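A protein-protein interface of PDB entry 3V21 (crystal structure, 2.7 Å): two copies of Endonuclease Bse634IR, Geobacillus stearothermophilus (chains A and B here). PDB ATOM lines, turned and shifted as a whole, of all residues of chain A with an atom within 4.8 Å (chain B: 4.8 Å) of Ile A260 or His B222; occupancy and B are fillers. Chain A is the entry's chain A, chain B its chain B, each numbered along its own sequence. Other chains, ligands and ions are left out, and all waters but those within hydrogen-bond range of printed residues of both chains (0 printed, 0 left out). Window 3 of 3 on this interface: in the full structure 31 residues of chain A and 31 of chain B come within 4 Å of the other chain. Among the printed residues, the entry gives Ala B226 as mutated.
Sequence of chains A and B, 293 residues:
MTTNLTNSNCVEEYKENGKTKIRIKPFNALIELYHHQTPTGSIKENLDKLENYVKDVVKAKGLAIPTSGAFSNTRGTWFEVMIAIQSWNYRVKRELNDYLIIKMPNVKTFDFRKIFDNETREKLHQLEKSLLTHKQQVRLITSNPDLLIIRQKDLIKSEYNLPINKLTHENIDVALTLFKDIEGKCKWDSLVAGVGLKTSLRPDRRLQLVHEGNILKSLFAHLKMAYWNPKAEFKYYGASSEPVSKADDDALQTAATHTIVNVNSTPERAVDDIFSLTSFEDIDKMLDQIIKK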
ATOM      1  N   ALA A 255      32.834 -29.224   5.801  1.00  0.00           N
ATOM      2  CA  ALA A 255      32.638 -28.689   4.460  1.00  0.00           C
ATOM      3  C   ALA A 255      33.557 -27.511   4.166  1.00  0.00           C
ATOM      4  O   ALA A 255      34.072 -26.865   5.077  1.00  0.00           O
ATOM      5  CB  ALA A 255      31.185 -28.286   4.262  1.00  0.00           C
ATOM      6  N   ALA A 256      33.755 -27.241   2.880  1.00  0.00           N
ATOM      7  CA  ALA A 256      34.535 -26.091   2.448  1.00  0.00           C
ATOM      8  C   ALA A 256      33.451 -25.025   2.522  1.00  0.00           C
ATOM      9  O   ALA A 256      32.637 -24.889   1.612  1.00  0.00           O
ATOM     10  CB  ALA A 256      35.121 -26.335   1.070  1.00  0.00           C
ATOM     11  N   THR A 257      33.445 -24.282   3.622  1.00  0.00           N
ATOM     12  CA  THR A 257      32.589 -23.112   3.786  1.00  0.00           C
ATOM     13  C   THR A 257      32.195 -22.258   2.584  1.00  0.00           C
ATOM     14  O   THR A 257      31.091 -21.720   2.533  1.00  0.00           O
ATOM     15  CB  THR A 257      33.288 -22.025   4.620  1.00  0.00           C
ATOM     16  OG1 THR A 257      33.582 -22.539   5.925  1.00  0.00           O
ATOM     17  CG2 THR A 257      32.393 -20.807   4.754  1.00  0.00           C
ATOM     18  N   HIS A 258      33.102 -22.105   1.635  1.00  0.00           N
ATOM     19  CA  HIS A 258      32.794 -21.488   0.349  1.00  0.00           C
ATOM     20  C   HIS A 258      31.986 -22.352  -0.618  1.00  0.00           C
ATOM     21  O   HIS A 258      31.548 -21.875  -1.662  1.00  0.00           O
ATOM     22  CB  HIS A 258      34.077 -20.990  -0.324  1.00  0.00           C
ATOM     23  CG  HIS A 258      35.014 -22.084  -0.728  1.00  0.00           C
ATOM     24  ND1 HIS A 258      36.051 -22.509   0.074  1.00  0.00           N
ATOM     25  CD2 HIS A 258      35.078 -22.835  -1.853  1.00  0.00           C
ATOM     26  CE1 HIS A 258      36.709 -23.478  -0.538  1.00  0.00           C
ATOM     27  NE2 HIS A 258      36.139 -23.695  -1.708  1.00  0.00           N
ATOM     28  N   THR A 259      31.785 -23.618  -0.270  1.00  0.00           N
ATOM     29  CA  THR A 259      31.018 -24.514  -1.122  1.00  0.00           C
ATOM     30  C   THR A 259      29.622 -24.814  -0.586  1.00  0.00           C
ATOM     31  O   THR A 259      28.889 -25.612  -1.174  1.00  0.00           O
ATOM     32  CB  THR A 259      31.716 -25.875  -1.308  1.00  0.00           C
ATOM     33  OG1 THR A 259      31.666 -26.609  -0.083  1.00  0.00           O
ATOM     34  CG2 THR A 259      33.156 -25.694  -1.716  1.00  0.00           C
ATOM     35  N   ILE A 260      29.250 -24.202   0.532  1.00  0.00           N
ATOM     36  CA  ILE A 260      27.920 -24.442   1.093  1.00  0.00           C
ATOM     37  C   ILE A 260      27.143 -23.151   1.316  1.00  0.00           C
ATOM     38  O   ILE A 260      26.168 -23.130   2.071  1.00  0.00           O
ATOM     39  CB  ILE A 260      27.992 -25.173   2.447  1.00  0.00           C
ATOM     40  CG1 ILE A 260      28.736 -24.309   3.476  1.00  0.00           C
ATOM     41  CG2 ILE A 260      28.670 -26.509   2.264  1.00  0.00           C
ATOM     42  CD1 ILE A 260      28.625 -24.801   4.911  1.00  0.00           C
ATOM     43  N   VAL A 261      27.583 -22.077   0.669  1.00  0.00           N
ATOM     44  CA  VAL A 261      26.934 -20.789   0.812  1.00  0.00           C
ATOM     45  C   VAL A 261      25.497 -20.839   0.314  1.00  0.00           C
ATOM     46  O   VAL A 261      24.573 -20.312   0.937  1.00  0.00           O
ATOM     47  CB  VAL A 261      27.673 -19.718   0.004  1.00  0.00           C
ATOM     48  CG1 VAL A 261      26.988 -18.372   0.162  1.00  0.00           C
ATOM     49  CG2 VAL A 261      29.103 -19.650   0.452  1.00  0.00           C
ATOM     50  N   ASN A 262      25.324 -21.522  -0.803  1.00  0.00           N
ATOM     51  CA  ASN A 262      24.054 -21.610  -1.473  1.00  0.00           C
ATOM     52  C   ASN A 262      23.314 -22.936  -1.308  1.00  0.00           C
ATOM     53  O   ASN A 262      23.940 -23.990  -1.290  1.00  0.00           O
ATOM     54  CB  ASN A 262      24.370 -21.351  -2.901  1.00  0.00           C
ATOM     55  CG  ASN A 262      24.558 -19.893  -3.229  1.00  0.00           C
ATOM     56  OD1 ASN A 262      23.994 -19.003  -2.591  1.00  0.00           O
ATOM     57  ND2 ASN A 262      25.358 -19.639  -4.261  1.00  0.00           N
ATOM     58  N   SER A 265      24.097 -24.830  -4.034  1.00  0.00           N
ATOM     59  CA  SER A 265      25.535 -25.066  -4.057  1.00  0.00           C
ATOM     60  C   SER A 265      25.730 -26.496  -3.513  1.00  0.00           C
ATOM     61  O   SER A 265      25.036 -26.896  -2.575  1.00  0.00           O
ATOM     62  CB  SER A 265      26.229 -24.039  -3.150  1.00  0.00           C
ATOM     63  OG  SER A 265      27.613 -23.943  -3.434  1.00  0.00           O
ATOM     64  N   PRO A 267      27.748 -29.354  -1.451  1.00  0.00           N
ATOM     65  CA  PRO A 267      28.796 -29.424  -0.433  1.00  0.00           C
ATOM     66  C   PRO A 267      30.041 -30.112  -0.947  1.00  0.00           C
ATOM     67  O   PRO A 267      29.979 -30.982  -1.818  1.00  0.00           O
ATOM     68  CB  PRO A 267      28.140 -30.214   0.700  1.00  0.00           C
ATOM     69  CG  PRO A 267      26.690 -29.947   0.510  1.00  0.00           C
ATOM     70  CD  PRO A 267      26.544 -30.058  -0.992  1.00  0.00           C
ATOM     71  N   LEU B 127      20.138 -27.475   8.225  1.00  0.00           N
ATOM     72  CA  LEU B 127      21.415 -27.393   7.537  1.00  0.00           C
ATOM     73  C   LEU B 127      22.325 -28.593   7.719  1.00  0.00           C
ATOM     74  O   LEU B 127      22.756 -29.214   6.752  1.00  0.00           O
ATOM     75  CB  LEU B 127      22.172 -26.136   7.980  1.00  0.00           C
ATOM     76  CG  LEU B 127      23.584 -25.983   7.408  1.00  0.00           C
ATOM     77  CD1 LEU B 127      23.526 -25.969   5.885  1.00  0.00           C
ATOM     78  CD2 LEU B 127      24.218 -24.710   7.945  1.00  0.00           C
ATOM     79  N   LEU B 131      23.478 -31.315   4.912  1.00  0.00           N
ATOM     80  CA  LEU B 131      24.860 -31.581   4.539  1.00  0.00           C
ATOM     81  C   LEU B 131      25.240 -33.049   4.619  1.00  0.00           C
ATOM     82  O   LEU B 131      26.139 -33.484   3.916  1.00  0.00           O
ATOM     83  CB  LEU B 131      25.809 -30.764   5.408  1.00  0.00           C
ATOM     84  CG  LEU B 131      25.660 -29.252   5.289  1.00  0.00           C
ATOM     85  CD1 LEU B 131      26.631 -28.571   6.248  1.00  0.00           C
ATOM     86  CD2 LEU B 131      25.920 -28.820   3.864  1.00  0.00           C
ATOM     87  N   LEU B 140      30.066 -29.511   9.673  1.00  0.00           N
ATOM     88  CA  LEU B 140      30.588 -28.191  10.016  1.00  0.00           C
ATOM     89  C   LEU B 140      31.056 -28.295  11.457  1.00  0.00           C
ATOM     90  O   LEU B 140      30.363 -27.872  12.383  1.00  0.00           O
ATOM     91  CB  LEU B 140      29.507 -27.115   9.897  1.00  0.00           C
ATOM     92  CG  LEU B 140      29.316 -26.509   8.511  1.00  0.00           C
ATOM     93  CD1 LEU B 140      28.230 -25.456   8.565  1.00  0.00           C
ATOM     94  CD2 LEU B 140      30.622 -25.889   8.048  1.00  0.00           C
ATOM     95  N   SER B 218      30.565 -19.171   9.244  1.00  0.00           N
ATOM     96  CA  SER B 218      29.858 -19.877   8.189  1.00  0.00           C
ATOM     97  C   SER B 218      28.488 -20.265   8.729  1.00  0.00           C
ATOM     98  O   SER B 218      27.475 -20.143   8.045  1.00  0.00           O
ATOM     99  CB  SER B 218      30.635 -21.122   7.766  1.00  0.00           C
ATOM    100  OG  SER B 218      29.956 -21.791   6.719  1.00  0.00           O
ATOM    101  N   LEU B 219      28.459 -20.739   9.967  1.00  0.00           N
ATOM    102  CA  LEU B 219      27.199 -21.106  10.597  1.00  0.00           C
ATOM    103  C   LEU B 219      26.344 -19.847  10.738  1.00  0.00           C
ATOM    104  O   LEU B 219      25.189 -19.824  10.329  1.00  0.00           O
ATOM    105  CB  LEU B 219      27.457 -21.709  11.978  1.00  0.00           C
ATOM    106  CG  LEU B 219      27.828 -23.190  12.024  1.00  0.00           C
ATOM    107  CD1 LEU B 219      28.479 -23.533  13.348  1.00  0.00           C
ATOM    108  CD2 LEU B 219      26.582 -24.015  11.822  1.00  0.00           C
ATOM    109  N   PHE B 220      26.922 -18.791  11.300  1.00  0.00           N
ATOM    110  CA  PHE B 220      26.186 -17.557  11.500  1.00  0.00           C
ATOM    111  C   PHE B 220      25.648 -17.032  10.181  1.00  0.00           C
ATOM    112  O   PHE B 220      24.538 -16.510  10.109  1.00  0.00           O
ATOM    113  CB  PHE B 220      27.080 -16.503  12.132  1.00  0.00           C
ATOM    114  CG  PHE B 220      26.321 -15.366  12.751  1.00  0.00           C
ATOM    115  CD1 PHE B 220      25.685 -15.523  13.983  1.00  0.00           C
ATOM    116  CD2 PHE B 220      26.224 -14.144  12.105  1.00  0.00           C
ATOM    117  CE1 PHE B 220      24.966 -14.481  14.560  1.00  0.00           C
ATOM    118  CE2 PHE B 220      25.506 -13.097  12.675  1.00  0.00           C
ATOM    119  CZ  PHE B 220      24.876 -13.269  13.908  1.00  0.00           C
ATOM    120  N   ALA B 221      26.443 -17.169   9.134  1.00  0.00           N
ATOM    121  CA  ALA B 221      26.037 -16.703   7.823  1.00  0.00           C
ATOM    122  C   ALA B 221      24.769 -17.407   7.399  1.00  0.00           C
ATOM    123  O   ALA B 221      23.915 -16.813   6.742  1.00  0.00           O
ATOM    124  CB  ALA B 221      27.129 -16.972   6.816  1.00  0.00           C
ATOM    125  N   HIS B 222      24.644 -18.677   7.767  1.00  0.00           N
ATOM    126  CA  HIS B 222      23.459 -19.424   7.393  1.00  0.00           C
ATOM    127  C   HIS B 222      22.247 -19.044   8.199  1.00  0.00           C
ATOM    128  O   HIS B 222      21.124 -19.197   7.721  1.00  0.00           O
ATOM    129  CB  HIS B 222      23.701 -20.925   7.482  1.00  0.00           C
ATOM    130  CG  HIS B 222      24.396 -21.480   6.279  1.00  0.00           C
ATOM    131  ND1 HIS B 222      25.693 -21.142   5.950  1.00  0.00           N
ATOM    132  CD2 HIS B 222      23.951 -22.283   5.280  1.00  0.00           C
ATOM    133  CE1 HIS B 222      26.016 -21.710   4.801  1.00  0.00           C
ATOM    134  NE2 HIS B 222      24.975 -22.406   4.372  1.00  0.00           N
ATOM    135  N   LEU B 223      22.459 -18.547   9.417  1.00  0.00           N
ATOM    136  CA  LEU B 223      21.348 -18.118  10.255  1.00  0.00           C
ATOM    137  C   LEU B 223      20.843 -16.794   9.694  1.00  0.00           C
ATOM    138  O   LEU B 223      19.639 -16.557   9.633  1.00  0.00           O
ATOM    139  CB  LEU B 223      21.798 -17.944  11.698  1.00  0.00           C
ATOM    140  CG  LEU B 223      22.105 -19.277  12.370  1.00  0.00           C
ATOM    141  CD1 LEU B 223      22.516 -19.054  13.805  1.00  0.00           C
ATOM    142  CD2 LEU B 223      20.873 -20.157  12.304  1.00  0.00           C
ATOM    143  N   LYS B 224      21.771 -15.936   9.278  1.00  0.00           N
ATOM    144  CA  LYS B 224      21.407 -14.664   8.679  1.00  0.00           C
ATOM    145  C   LYS B 224      20.547 -14.934   7.443  1.00  0.00           C
ATOM    146  O   LYS B 224      19.582 -14.217   7.197  1.00  0.00           O
ATOM    147  CB  LYS B 224      22.651 -13.885   8.277  1.00  0.00           C
ATOM    148  CG  LYS B 224      23.480 -13.424   9.443  1.00  0.00           C
ATOM    149  CD  LYS B 224      24.666 -12.589   8.984  1.00  0.00           C
ATOM    150  CE  LYS B 224      24.210 -11.373   8.223  1.00  0.00           C
ATOM    151  NZ  LYS B 224      25.354 -10.496   7.911  1.00  0.00           N
ATOM    152  N   MET B 225      20.893 -15.961   6.665  1.00  0.00           N
ATOM    153  CA  MET B 225      20.110 -16.316   5.477  1.00  0.00           C
ATOM    154  C   MET B 225      18.741 -16.738   5.967  1.00  0.00           C
ATOM    155  O   MET B 225      17.720 -16.164   5.594  1.00  0.00           O
ATOM    156  CB  MET B 225      20.724 -17.504   4.742  1.00  0.00           C
ATOM    157  CG  MET B 225      22.004 -17.222   3.988  1.00  0.00           C
ATOM    158  SD  MET B 225      21.741 -16.517   2.335  1.00  0.00           S
ATOM    159  CE  MET B 225      23.376 -15.700   2.051  1.00  0.00           C
ATOM    160  N   ALA B 226      18.751 -17.754   6.821  1.00  0.00           N
ATOM    161  CA  ALA B 226      17.542 -18.330   7.393  1.00  0.00           C
ATOM    162  C   ALA B 226      16.530 -17.278   7.810  1.00  0.00           C
ATOM    163  O   ALA B 226      15.343 -17.362   7.477  1.00  0.00           O
ATOM    164  CB  ALA B 226      17.903 -19.203   8.581  1.00  0.00           C
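The backbone carbonyl oxygen (O) of Ile A260 is in hydrogen-bond range of a ring nitrogen (NE2) of His B222.
Of chain B, only Leu B131, Leu B140, Ser B218 and His B222 come within 4 Å of Ile A260.
Printed residues of chain A within 4 Å of Leu B131: Ile A260 and Pro A267.
Printed residues of chain A within 4 Å of Leu B140: Ile A260 (3.7 Å).
His B222 touches just one residue of chain A: Ile A260.
Lys B224 touches none of the printed residues of chain A.
Ala B226 touches none of the printed residues of chain A.
The nearest printed residue of chain B that does not touch Ile A260 is Leu B127 (5.3 Å).
No position is printed for both chains.
Of the 6 pairs that touch across the chains among the printed residues, none has its exchanged pair printed and touching as well.
The backbone carbonyl oxygen (O) of Ser B218 is in hydrogen-bond range of a ring nitrogen (ND1) of His B222 (2.9 Å).
Hydrophobic or aromatic side chains of chain A within 4 Å of the printed part of chain B: Ile A260 and Pro A267.
Of the 12 printed residues of chain B, 4 touch a printed residue of chain A.
Among the printed residues, 6 pairs touch across the chains.
Among the printed residues, no Asp or Glu carboxylate lies within 4 Å of a Lys or Arg side-chain nitrogen of the other chain.
CG2 of Thr A257 touches OG of Ser B218, 3.3 Å away.
Ile A260 touches Leu B131 (CG2 to CD2, 3.9 Å).
Ile A260 touches Leu B140.
CD1 of Ile A260 touches OG of Ser B218, 3.8 Å away.
CG of Pro A267 touches CD2 of Leu B131 (3.6 Å).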
